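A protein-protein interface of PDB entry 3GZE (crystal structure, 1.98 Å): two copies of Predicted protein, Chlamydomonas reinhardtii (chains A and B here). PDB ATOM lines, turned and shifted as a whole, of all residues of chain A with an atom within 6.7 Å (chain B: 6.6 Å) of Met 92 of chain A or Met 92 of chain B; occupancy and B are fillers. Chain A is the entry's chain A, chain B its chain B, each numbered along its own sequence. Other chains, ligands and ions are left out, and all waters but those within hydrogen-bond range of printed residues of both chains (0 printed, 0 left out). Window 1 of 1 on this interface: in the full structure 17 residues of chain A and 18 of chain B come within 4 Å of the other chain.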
ATOM      1  N   TRP A  19      18.783  -4.241  28.178  1.00  0.00           N
ATOM      2  CA  TRP A  19      19.948  -4.270  27.305  1.00  0.00           C
ATOM      3  C   TRP A  19      21.163  -4.868  27.984  1.00  0.00           C
ATOM      4  O   TRP A  19      22.004  -5.531  27.369  1.00  0.00           O
ATOM      5  CB  TRP A  19      20.274  -2.875  26.790  1.00  0.00           C
ATOM      6  CG  TRP A  19      19.450  -2.532  25.548  1.00  0.00           C
ATOM      7  CD1 TRP A  19      18.564  -1.491  25.404  1.00  0.00           C
ATOM      8  CD2 TRP A  19      19.402  -3.274  24.310  1.00  0.00           C
ATOM      9  NE1 TRP A  19      18.013  -1.519  24.118  1.00  0.00           N
ATOM     10  CE2 TRP A  19      18.504  -2.615  23.449  1.00  0.00           C
ATOM     11  CE3 TRP A  19      20.044  -4.414  23.843  1.00  0.00           C
ATOM     12  CZ2 TRP A  19      18.235  -3.078  22.154  1.00  0.00           C
ATOM     13  CZ3 TRP A  19      19.797  -4.840  22.548  1.00  0.00           C
ATOM     14  CH2 TRP A  19      18.887  -4.197  21.742  1.00  0.00           C
ATOM     15  N   ARG A  22      21.192  -8.483  27.951  1.00  0.00           N
ATOM     16  CA  ARG A  22      20.328  -8.454  26.765  1.00  0.00           C
ATOM     17  C   ARG A  22      19.295  -9.475  26.996  1.00  0.00           C
ATOM     18  O   ARG A  22      19.584 -10.679  26.971  1.00  0.00           O
ATOM     19  CB  ARG A  22      21.064  -8.787  25.461  1.00  0.00           C
ATOM     20  CG  ARG A  22      21.971  -7.658  25.059  1.00  0.00           C
ATOM     21  CD  ARG A  22      22.631  -7.915  23.723  1.00  0.00           C
ATOM     22  NE  ARG A  22      23.667  -8.932  23.771  1.00  0.00           N
ATOM     23  CZ  ARG A  22      23.986  -9.687  22.746  1.00  0.00           C
ATOM     24  NH1 ARG A  22      23.273  -9.632  21.609  1.00  0.00           N
ATOM     25  NH2 ARG A  22      24.988 -10.509  22.848  1.00  0.00           N
ATOM     26  N   PHE A  24      15.043 -10.422  26.406  1.00  0.00           N
ATOM     27  CA  PHE A  24      13.806 -10.299  25.654  1.00  0.00           C
ATOM     28  C   PHE A  24      12.789 -11.349  26.124  1.00  0.00           C
ATOM     29  O   PHE A  24      13.125 -12.481  26.320  1.00  0.00           O
ATOM     30  CB  PHE A  24      14.137 -10.469  24.162  1.00  0.00           C
ATOM     31  CG  PHE A  24      15.251  -9.571  23.699  1.00  0.00           C
ATOM     32  CD1 PHE A  24      16.562  -9.965  23.759  1.00  0.00           C
ATOM     33  CD2 PHE A  24      14.995  -8.333  23.217  1.00  0.00           C
ATOM     34  CE1 PHE A  24      17.574  -9.126  23.350  1.00  0.00           C
ATOM     35  CE2 PHE A  24      16.049  -7.491  22.817  1.00  0.00           C
ATOM     36  CZ  PHE A  24      17.307  -7.918  22.893  1.00  0.00           C
ATOM     37  N   VAL A  87      12.895 -22.188  17.951  1.00  0.00           N
ATOM     38  CA  VAL A  87      13.971 -21.589  18.822  1.00  0.00           C
ATOM     39  C   VAL A  87      15.179 -21.150  17.981  1.00  0.00           C
ATOM     40  O   VAL A  87      15.799 -20.141  18.200  1.00  0.00           O
ATOM     41  CB  VAL A  87      14.416 -22.538  20.028  1.00  0.00           C
ATOM     42  CG1 VAL A  87      15.749 -22.015  20.685  1.00  0.00           C
ATOM     43  CG2 VAL A  87      13.278 -22.699  21.113  1.00  0.00           C
ATOM     44  N   ALA A  88      15.500 -21.946  16.984  1.00  0.00           N
ATOM     45  CA  ALA A  88      16.611 -21.619  16.027  1.00  0.00           C
ATOM     46  C   ALA A  88      16.250 -20.421  15.191  1.00  0.00           C
ATOM     47  O   ALA A  88      17.043 -19.537  14.915  1.00  0.00           O
ATOM     48  CB  ALA A  88      16.997 -22.814  15.154  1.00  0.00           C
ATOM     49  N   GLN A  89      14.985 -20.334  14.897  1.00  0.00           N
ATOM     50  CA  GLN A  89      14.417 -19.226  14.066  1.00  0.00           C
ATOM     51  C   GLN A  89      14.584 -17.886  14.765  1.00  0.00           C
ATOM     52  O   GLN A  89      15.051 -16.863  14.189  1.00  0.00           O
ATOM     53  CB  GLN A  89      12.909 -19.404  13.809  1.00  0.00           C
ATOM     54  CG  GLN A  89      12.560 -20.232  12.579  1.00  0.00           C
ATOM     55  CD  GLN A  89      11.090 -20.169  12.191  1.00  0.00           C
ATOM     56  OE1 GLN A  89      10.196 -20.329  13.026  1.00  0.00           O
ATOM     57  NE2 GLN A  89      10.836 -19.961  10.903  1.00  0.00           N
ATOM     58  N   VAL A  90      14.148 -17.900  16.010  1.00  0.00           N
ATOM     59  CA  VAL A  90      14.093 -16.674  16.823  1.00  0.00           C
ATOM     60  C   VAL A  90      15.456 -16.231  17.333  1.00  0.00           C
ATOM     61  O   VAL A  90      15.748 -15.044  17.405  1.00  0.00           O
ATOM     62  CB  VAL A  90      13.011 -16.667  17.886  1.00  0.00           C
ATOM     63  CG1 VAL A  90      11.685 -16.883  17.164  1.00  0.00           C
ATOM     64  CG2 VAL A  90      13.311 -17.685  19.011  1.00  0.00           C
ATOM     65  N   THR A  91      16.286 -17.197  17.673  1.00  0.00           N
ATOM     66  CA  THR A  91      17.670 -16.875  18.124  1.00  0.00           C
ATOM     67  C   THR A  91      18.643 -16.597  16.983  1.00  0.00           C
ATOM     68  O   THR A  91      19.693 -15.989  17.143  1.00  0.00           O
ATOM     69  CB  THR A  91      18.257 -17.985  18.956  1.00  0.00           C
ATOM     70  OG1 THR A  91      18.282 -19.193  18.187  1.00  0.00           O
ATOM     71  CG2 THR A  91      17.428 -18.185  20.213  1.00  0.00           C
ATOM     72  N   MET A  92      18.242 -17.073  15.833  1.00  0.00           N
ATOM     73  CA  MET A  92      18.993 -16.967  14.592  1.00  0.00           C
ATOM     74  C   MET A  92      20.321 -17.688  14.663  1.00  0.00           C
ATOM     75  O   MET A  92      21.272 -17.320  14.005  1.00  0.00           O
ATOM     76  CB  MET A  92      19.201 -15.493  14.152  1.00  0.00           C
ATOM     77  CG  MET A  92      17.908 -14.769  13.809  1.00  0.00           C
ATOM     78  SD  MET A  92      17.987 -13.005  13.428  1.00  0.00           S
ATOM     79  CE  MET A  92      18.232 -12.388  15.092  1.00  0.00           C
ATOM     80  N   ILE A  93      20.348 -18.732  15.479  1.00  0.00           N
ATOM     81  CA  ILE A  93      21.481 -19.670  15.505  1.00  0.00           C
ATOM     82  C   ILE A  93      21.079 -21.105  15.070  1.00  0.00           C
ATOM     83  O   ILE A  93      20.052 -21.592  15.517  1.00  0.00           O
ATOM     84  CB  ILE A  93      22.150 -19.641  16.907  1.00  0.00           C
ATOM     85  CG1 ILE A  93      22.543 -18.193  17.231  1.00  0.00           C
ATOM     86  CG2 ILE A  93      23.427 -20.645  17.048  1.00  0.00           C
ATOM     87  CD1 ILE A  93      22.851 -18.025  18.690  1.00  0.00           C
ATOM     88  N   PRO A  94      21.926 -21.795  14.247  1.00  0.00           N
ATOM     89  CA  PRO A  94      21.454 -23.060  13.710  1.00  0.00           C
ATOM     90  C   PRO A  94      21.393 -24.145  14.741  1.00  0.00           C
ATOM     91  O   PRO A  94      22.157 -24.178  15.695  1.00  0.00           O
ATOM     92  CB  PRO A  94      22.488 -23.407  12.652  1.00  0.00           C
ATOM     93  CG  PRO A  94      23.702 -22.770  13.101  1.00  0.00           C
ATOM     94  CD  PRO A  94      23.265 -21.464  13.725  1.00  0.00           C
ATOM     95  N   HIS A  98      22.757 -26.153  19.325  1.00  0.00           N
ATOM     96  CA  HIS A  98      21.830 -26.261  20.456  1.00  0.00           C
ATOM     97  C   HIS A  98      22.040 -27.552  21.233  1.00  0.00           C
ATOM     98  O   HIS A  98      22.105 -28.661  20.673  1.00  0.00           O
ATOM     99  CB  HIS A  98      20.338 -26.224  20.002  1.00  0.00           C
ATOM    100  CG  HIS A  98      19.962 -25.001  19.244  1.00  0.00           C
ATOM    101  ND1 HIS A  98      18.737 -24.387  19.372  1.00  0.00           N
ATOM    102  CD2 HIS A  98      20.660 -24.262  18.356  1.00  0.00           C
ATOM    103  CE1 HIS A  98      18.700 -23.332  18.573  1.00  0.00           C
ATOM    104  NE2 HIS A  98      19.852 -23.237  17.944  1.00  0.00           N
ATOM    105  N   MET A 183      14.327 -14.988  26.502  1.00  0.00           N
ATOM    106  CA  MET A 183      15.612 -15.123  25.814  1.00  0.00           C
ATOM    107  C   MET A 183      16.576 -14.114  26.423  1.00  0.00           C
ATOM    108  O   MET A 183      16.293 -12.922  26.451  1.00  0.00           O
ATOM    109  CB  MET A 183      15.478 -14.783  24.347  1.00  0.00           C
ATOM    110  CG  MET A 183      16.763 -15.002  23.504  1.00  0.00           C
ATOM    111  SD  MET A 183      16.589 -14.372  21.828  1.00  0.00           S
ATOM    112  CE  MET A 183      15.191 -15.179  21.244  1.00  0.00           C
ATOM    113  N   TYR A 185      21.101 -13.282  26.656  1.00  0.00           N
ATOM    114  CA  TYR A 185      22.490 -13.621  26.202  1.00  0.00           C
ATOM    115  C   TYR A 185      23.486 -13.725  27.323  1.00  0.00           C
ATOM    116  O   TYR A 185      23.537 -12.852  28.177  1.00  0.00           O
ATOM    117  CB  TYR A 185      22.975 -12.601  25.202  1.00  0.00           C
ATOM    118  CG  TYR A 185      22.237 -12.642  23.912  1.00  0.00           C
ATOM    119  CD1 TYR A 185      22.814 -13.186  22.768  1.00  0.00           C
ATOM    120  CD2 TYR A 185      20.931 -12.097  23.807  1.00  0.00           C
ATOM    121  CE1 TYR A 185      22.099 -13.214  21.499  1.00  0.00           C
ATOM    122  CE2 TYR A 185      20.256 -12.129  22.590  1.00  0.00           C
ATOM    123  CZ  TYR A 185      20.854 -12.665  21.444  1.00  0.00           C
ATOM    124  OH  TYR A 185      20.117 -12.657  20.260  1.00  0.00           O
ATOM    125  N   PRO A 189      28.109  -9.061  22.333  1.00  0.00           N
ATOM    126  CA  PRO A 189      28.146  -9.420  20.899  1.00  0.00           C
ATOM    127  C   PRO A 189      29.529  -9.718  20.335  1.00  0.00           C
ATOM    128  O   PRO A 189      29.680 -10.282  19.222  1.00  0.00           O
ATOM    129  CB  PRO A 189      27.513  -8.200  20.200  1.00  0.00           C
ATOM    130  CG  PRO A 189      26.725  -7.515  21.269  1.00  0.00           C
ATOM    131  CD  PRO A 189      27.461  -7.762  22.564  1.00  0.00           C
ATOM    132  N   TRP B  19      20.854 -20.445   6.002  1.00  0.00           N
ATOM    133  CA  TRP B  19      21.723 -20.749   7.169  1.00  0.00           C
ATOM    134  C   TRP B  19      23.215 -20.519   6.867  1.00  0.00           C
ATOM    135  O   TRP B  19      23.996 -20.184   7.734  1.00  0.00           O
ATOM    136  CB  TRP B  19      21.486 -22.158   7.713  1.00  0.00           C
ATOM    137  CG  TRP B  19      20.250 -22.283   8.556  1.00  0.00           C
ATOM    138  CD1 TRP B  19      19.220 -23.100   8.311  1.00  0.00           C
ATOM    139  CD2 TRP B  19      19.943 -21.594   9.792  1.00  0.00           C
ATOM    140  NE1 TRP B  19      18.287 -23.000   9.302  1.00  0.00           N
ATOM    141  CE2 TRP B  19      18.707 -22.071  10.225  1.00  0.00           C
ATOM    142  CE3 TRP B  19      20.596 -20.614  10.562  1.00  0.00           C
ATOM    143  CZ2 TRP B  19      18.074 -21.586  11.371  1.00  0.00           C
ATOM    144  CZ3 TRP B  19      19.996 -20.146  11.685  1.00  0.00           C
ATOM    145  CH2 TRP B  19      18.729 -20.629  12.093  1.00  0.00           C
ATOM    146  N   ARG B  22      23.848 -16.808   7.237  1.00  0.00           N
ATOM    147  CA  ARG B  22      22.613 -16.568   8.036  1.00  0.00           C
ATOM    148  C   ARG B  22      21.928 -15.325   7.527  1.00  0.00           C
ATOM    149  O   ARG B  22      22.422 -14.240   7.648  1.00  0.00           O
ATOM    150  CB  ARG B  22      22.893 -16.466   9.529  1.00  0.00           C
ATOM    151  CG  ARG B  22      23.284 -17.761  10.186  1.00  0.00           C
ATOM    152  CD  ARG B  22      23.591 -17.574  11.674  1.00  0.00           C
ATOM    153  NE  ARG B  22      24.733 -16.691  11.971  1.00  0.00           N
ATOM    154  CZ  ARG B  22      24.843 -15.994  13.096  1.00  0.00           C
ATOM    155  NH1 ARG B  22      23.867 -16.022  13.967  1.00  0.00           N
ATOM    156  NH2 ARG B  22      25.921 -15.246  13.354  1.00  0.00           N
ATOM    157  N   PHE B  24      17.926 -13.421   6.570  1.00  0.00           N
ATOM    158  CA  PHE B  24      16.523 -13.246   6.991  1.00  0.00           C
ATOM    159  C   PHE B  24      15.893 -12.019   6.375  1.00  0.00           C
ATOM    160  O   PHE B  24      16.529 -10.964   6.231  1.00  0.00           O
ATOM    161  CB  PHE B  24      16.399 -13.180   8.548  1.00  0.00           C
ATOM    162  CG  PHE B  24      17.070 -14.333   9.245  1.00  0.00           C
ATOM    163  CD1 PHE B  24      18.403 -14.315   9.506  1.00  0.00           C
ATOM    164  CD2 PHE B  24      16.351 -15.447   9.619  1.00  0.00           C
ATOM    165  CE1 PHE B  24      19.009 -15.398  10.118  1.00  0.00           C
ATOM    166  CE2 PHE B  24      16.940 -16.491  10.217  1.00  0.00           C
ATOM    167  CZ  PHE B  24      18.307 -16.471  10.432  1.00  0.00           C
ATOM    168  N   VAL B  87      15.528  -1.540  14.473  1.00  0.00           N
ATOM    169  CA  VAL B  87      16.739  -2.299  14.025  1.00  0.00           C
ATOM    170  C   VAL B  87      17.440  -2.864  15.227  1.00  0.00           C
ATOM    171  O   VAL B  87      17.789  -4.042  15.275  1.00  0.00           O
ATOM    172  CB  VAL B  87      17.756  -1.461  13.195  1.00  0.00           C
ATOM    173  CG1 VAL B  87      19.049  -2.362  12.849  1.00  0.00           C
ATOM    174  CG2 VAL B  87      17.122  -0.832  11.921  1.00  0.00           C
ATOM    175  N   ALA B  88      17.667  -2.014  16.219  1.00  0.00           N
ATOM    176  CA  ALA B  88      18.271  -2.516  17.500  1.00  0.00           C
ATOM    177  C   ALA B  88      17.486  -3.704  18.078  1.00  0.00           C
ATOM    178  O   ALA B  88      18.042  -4.741  18.518  1.00  0.00           O
ATOM    179  CB  ALA B  88      18.346  -1.419  18.509  1.00  0.00           C
ATOM    180  N   GLN B  89      16.175  -3.570  18.014  1.00  0.00           N
ATOM    181  CA  GLN B  89      15.295  -4.599  18.621  1.00  0.00           C
ATOM    182  C   GLN B  89      15.408  -5.909  17.886  1.00  0.00           C
ATOM    183  O   GLN B  89      15.693  -6.927  18.513  1.00  0.00           O
ATOM    184  CB  GLN B  89      13.856  -4.160  18.815  1.00  0.00           C
ATOM    185  CG  GLN B  89      13.755  -3.012  19.802  1.00  0.00           C
ATOM    186  CD  GLN B  89      13.984  -3.349  21.298  1.00  0.00           C
ATOM    187  OE1 GLN B  89      14.355  -4.480  21.669  1.00  0.00           O
ATOM    188  NE2 GLN B  89      13.760  -2.344  22.168  1.00  0.00           N
ATOM    189  N   VAL B  90      15.315  -5.870  16.549  1.00  0.00           N
ATOM    190  CA  VAL B  90      15.222  -7.126  15.754  1.00  0.00           C
ATOM    191  C   VAL B  90      16.570  -7.870  15.674  1.00  0.00           C
ATOM    192  O   VAL B  90      16.612  -9.076  15.526  1.00  0.00           O
ATOM    193  CB  VAL B  90      14.494  -6.991  14.338  1.00  0.00           C
ATOM    194  CG1 VAL B  90      13.101  -6.419  14.537  1.00  0.00           C
ATOM    195  CG2 VAL B  90      15.287  -6.148  13.252  1.00  0.00           C
ATOM    196  N   THR B  91      17.670  -7.114  15.716  1.00  0.00           N
ATOM    197  CA  THR B  91      19.033  -7.642  15.680  1.00  0.00           C
ATOM    198  C   THR B  91      19.558  -8.073  17.048  1.00  0.00           C
ATOM    199  O   THR B  91      20.480  -8.881  17.194  1.00  0.00           O
ATOM    200  CB  THR B  91      20.043  -6.633  15.060  1.00  0.00           C
ATOM    201  OG1 THR B  91      20.100  -5.443  15.850  1.00  0.00           O
ATOM    202  CG2 THR B  91      19.615  -6.241  13.626  1.00  0.00           C
ATOM    203  N   MET B  92      18.862  -7.579  18.017  1.00  0.00           N
ATOM    204  CA  MET B  92      19.154  -7.700  19.412  1.00  0.00           C
ATOM    205  C   MET B  92      20.559  -7.317  19.817  1.00  0.00           C
ATOM    206  O   MET B  92      21.097  -7.805  20.786  1.00  0.00           O
ATOM    207  CB  MET B  92      18.779  -9.103  19.893  1.00  0.00           C
ATOM    208  CG  MET B  92      17.311  -9.430  19.805  1.00  0.00           C
ATOM    209  SD  MET B  92      17.001 -11.207  20.195  1.00  0.00           S
ATOM    210  CE  MET B  92      17.589 -11.900  18.762  1.00  0.00           C
ATOM    211  N   ILE B  93      21.069  -6.327  19.114  1.00  0.00           N
ATOM    212  CA  ILE B  93      22.350  -5.629  19.406  1.00  0.00           C
ATOM    213  C   ILE B  93      22.063  -4.139  19.626  1.00  0.00           C
ATOM    214  O   ILE B  93      21.447  -3.506  18.784  1.00  0.00           O
ATOM    215  CB  ILE B  93      23.326  -5.770  18.204  1.00  0.00           C
ATOM    216  CG1 ILE B  93      23.512  -7.253  17.881  1.00  0.00           C
ATOM    217  CG2 ILE B  93      24.631  -5.039  18.438  1.00  0.00           C
ATOM    218  CD1 ILE B  93      24.232  -7.502  16.595  1.00  0.00           C
ATOM    219  N   PRO B  94      22.543  -3.569  20.747  1.00  0.00           N
ATOM    220  CA  PRO B  94      22.106  -2.251  21.044  1.00  0.00           C
ATOM    221  C   PRO B  94      22.673  -1.206  20.139  1.00  0.00           C
ATOM    222  O   PRO B  94      23.705  -1.396  19.498  1.00  0.00           O
ATOM    223  CB  PRO B  94      22.652  -2.036  22.468  1.00  0.00           C
ATOM    224  CG  PRO B  94      23.854  -2.865  22.514  1.00  0.00           C
ATOM    225  CD  PRO B  94      23.475  -4.082  21.771  1.00  0.00           C
ATOM    226  N   HIS B  98      25.815   0.415  16.477  1.00  0.00           N
ATOM    227  CA  HIS B  98      25.358   0.672  15.089  1.00  0.00           C
ATOM    228  C   HIS B  98      26.061   1.876  14.489  1.00  0.00           C
ATOM    229  O   HIS B  98      26.365   2.831  15.185  1.00  0.00           O
ATOM    230  CB  HIS B  98      23.875   0.943  15.069  1.00  0.00           C
ATOM    231  CG  HIS B  98      23.049  -0.183  15.634  1.00  0.00           C
ATOM    232  ND1 HIS B  98      21.776  -0.473  15.195  1.00  0.00           N
ATOM    233  CD2 HIS B  98      23.283  -1.021  16.670  1.00  0.00           C
ATOM    234  CE1 HIS B  98      21.289  -1.498  15.886  1.00  0.00           C
ATOM    235  NE2 HIS B  98      22.186  -1.848  16.788  1.00  0.00           N
ATOM    236  N   MET B 183      18.270  -8.852   6.332  1.00  0.00           N
ATOM    237  CA  MET B 183      19.187  -9.015   7.473  1.00  0.00           C
ATOM    238  C   MET B 183      20.067 -10.227   7.240  1.00  0.00           C
ATOM    239  O   MET B 183      19.588 -11.331   7.036  1.00  0.00           O
ATOM    240  CB  MET B 183      18.415  -9.208   8.794  1.00  0.00           C
ATOM    241  CG  MET B 183      19.282  -9.124  10.080  1.00  0.00           C
ATOM    242  SD  MET B 183      18.562  -9.814  11.649  1.00  0.00           S
ATOM    243  CE  MET B 183      17.241  -8.689  11.953  1.00  0.00           C
ATOM    244  N   TYR B 185      24.170 -11.917   8.477  1.00  0.00           N
ATOM    245  CA  TYR B 185      25.334 -12.018   9.395  1.00  0.00           C
ATOM    246  C   TYR B 185      26.626 -12.145   8.608  1.00  0.00           C
ATOM    247  O   TYR B 185      26.758 -12.979   7.705  1.00  0.00           O
ATOM    248  CB  TYR B 185      25.192 -13.206  10.351  1.00  0.00           C
ATOM    249  CG  TYR B 185      24.209 -12.937  11.418  1.00  0.00           C
ATOM    250  CD1 TYR B 185      24.611 -12.361  12.644  1.00  0.00           C
ATOM    251  CD2 TYR B 185      22.856 -13.196  11.208  1.00  0.00           C
ATOM    252  CE1 TYR B 185      23.691 -12.100  13.633  1.00  0.00           C
ATOM    253  CE2 TYR B 185      21.942 -12.947  12.178  1.00  0.00           C
ATOM    254  CZ  TYR B 185      22.359 -12.390  13.404  1.00  0.00           C
ATOM    255  OH  TYR B 185      21.423 -12.116  14.383  1.00  0.00           O
ATOM    256  N   PRO B 189      28.480 -17.380  14.570  1.00  0.00           N
ATOM    257  CA  PRO B 189      28.177 -17.114  15.977  1.00  0.00           C
ATOM    258  C   PRO B 189      29.378 -17.003  16.942  1.00  0.00           C
ATOM    259  O   PRO B 189      29.303 -16.386  18.020  1.00  0.00           O
ATOM    260  CB  PRO B 189      27.243 -18.250  16.332  1.00  0.00           C
ATOM    261  CG  PRO B 189      26.539 -18.521  15.064  1.00  0.00           C
ATOM    262  CD  PRO B 189      27.627 -18.461  14.044  1.00  0.00           C
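The guanidinium group of Arg 22 of chain A sits at hydrogen-bond distance from the backbone carbonyl oxygen of Met 92 of chain B (3.0 Å). The guanidinium group of Arg 22 of chain B sits at hydrogen-bond distance from the backbone carbonyl oxygen of Met 92 of chain A (2.9 Å). SD of Met 92 of chain A sits close to OH of Tyr 185 of chain B (3.7 Å). SD of Met 92 of chain B sits close to OH of Tyr 185 of chain A (3.4 Å). The side-chain sulfur (SD) of Met 183 of chain B lies close to the side-chain sulfur (SD) of Met 92 of chain A (3.7 Å). The side-chain sulfur (SD) of Met 183 of chain A sits close to the side-chain sulfur (SD) of Met 92 of chain B (3.6 Å).
Of the 15 printed residues of chain A, 10 touch a printed residue of chain B. Hydrophobic or aromatic side chains of chain B within 4 Å of the printed part of chain A: Trp 19, Phe 24, Met 92, Pro 94, Met 183 and Tyr 185. Among the printed residues, 20 pairs touch across the chains.
O of Arg 22 of chain A sits at hydrogen-bond distance from N of Tyr 185 of chain A (3.0 Å). N of Met 183 of chain A lies within hydrogen-bond range of O of Phe 24 of chain A. A ring nitrogen (NE2) of His 98 of chain A lies within hydrogen-bond range of the backbone carbonyl oxygen (O) of Ile 93 of chain A. A ring nitrogen (NE2) of His 98 of chain A lies close to the backbone carbonyl oxygen (O) of Pro 94 of chain A. The backbone NH (N) of Tyr 185 of chain B is in hydrogen-bond range of the backbone carbonyl oxygen (O) of Arg 22 of chain B (3.0 Å). O of Ile 93 of chain B is in hydrogen-bond range of NE2 of His 98 of chain B, at 2.7 Å.
Met 92 of chain A touches just these residues of chain B: Trp 19 (3.9 Å), Arg 22 (2.9 Å), Phe 24 (3.8 Å), Val 90 (3.7 Å), Met 92 (3.8 Å), Met 183 (3.7 Å) and Tyr 185 (3.3 Å). Of the printed residues of chain A, Arg 22 of chain B touches Met 92. Printed residues of chain A within 4 Å of Phe 24 of chain B: Met 92 (3.8 Å). Val 87 of chain B touches none of the printed residues of chain A. Of chain A, only Trp 19, Arg 22, Phe 24, Val 90, Met 92, Met 183 and Tyr 185 come within 4 Å of Met 92 of chain B. Of the printed residues of chain A, Ile 93 of chain B touches Trp 19 (3.8 Å). The nearest printed residue of chain B that does not touch Trp 19 of chain A is Gln 89 of chain B (4.2 Å).
Among the printed residues, pairs that only touch across the chains: Trp 19 of chain A with Ala 88 of chain B (3.4 Å), Trp 19 of chain A with Met 92 of chain B (3.7 Å), Trp 19 of chain A with Ile 93 of chain B (3.8 Å), Trp 19 of chain A with Pro 94 of chain B (3.5 Å), Phe 24 of chain A with Gln 89 of chain B (3.6 Å), Phe 24 of chain A with Met 92 of chain B (3.4 Å), Ala 88 of chain A with Trp 19 of chain B (3.5 Å), Val 90 of chain A with Met 92 of chain B (3.9 Å), Met 92 of chain A with Trp 19 of chain B (3.9 Å), Met 92 of chain A with Phe 24 of chain B (3.8 Å), Met 92 of chain A with Val 90 of chain B (3.7 Å), Met 92 of chain A with Met 92 of chain B (3.8 Å), Ile 93 of chain A with Trp 19 of chain B (3.7 Å) and Pro 94 of chain A with Trp 19 of chain B (3.6 Å).
Trp 19 of chain A touches Pro 94 of chain B, and with the chains exchanged Pro 94 of chain A touches Trp 19 of chain B. Arg 22 of chain A touches Met 92 of chain B, and with the chains exchanged Met 92 of chain A touches Arg 22 of chain B. Phe 24 of chain A touches Gln 89 of chain B, but with the chains exchanged Gln 89 of chain A does not touch Phe 24 of chain B (4.4 Å). Phe 24 of chain A touches Met 92 of chain B, and with the chains exchanged Met 92 of chain A touches Phe 24 of chain B. 15 positions are printed for both chains.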
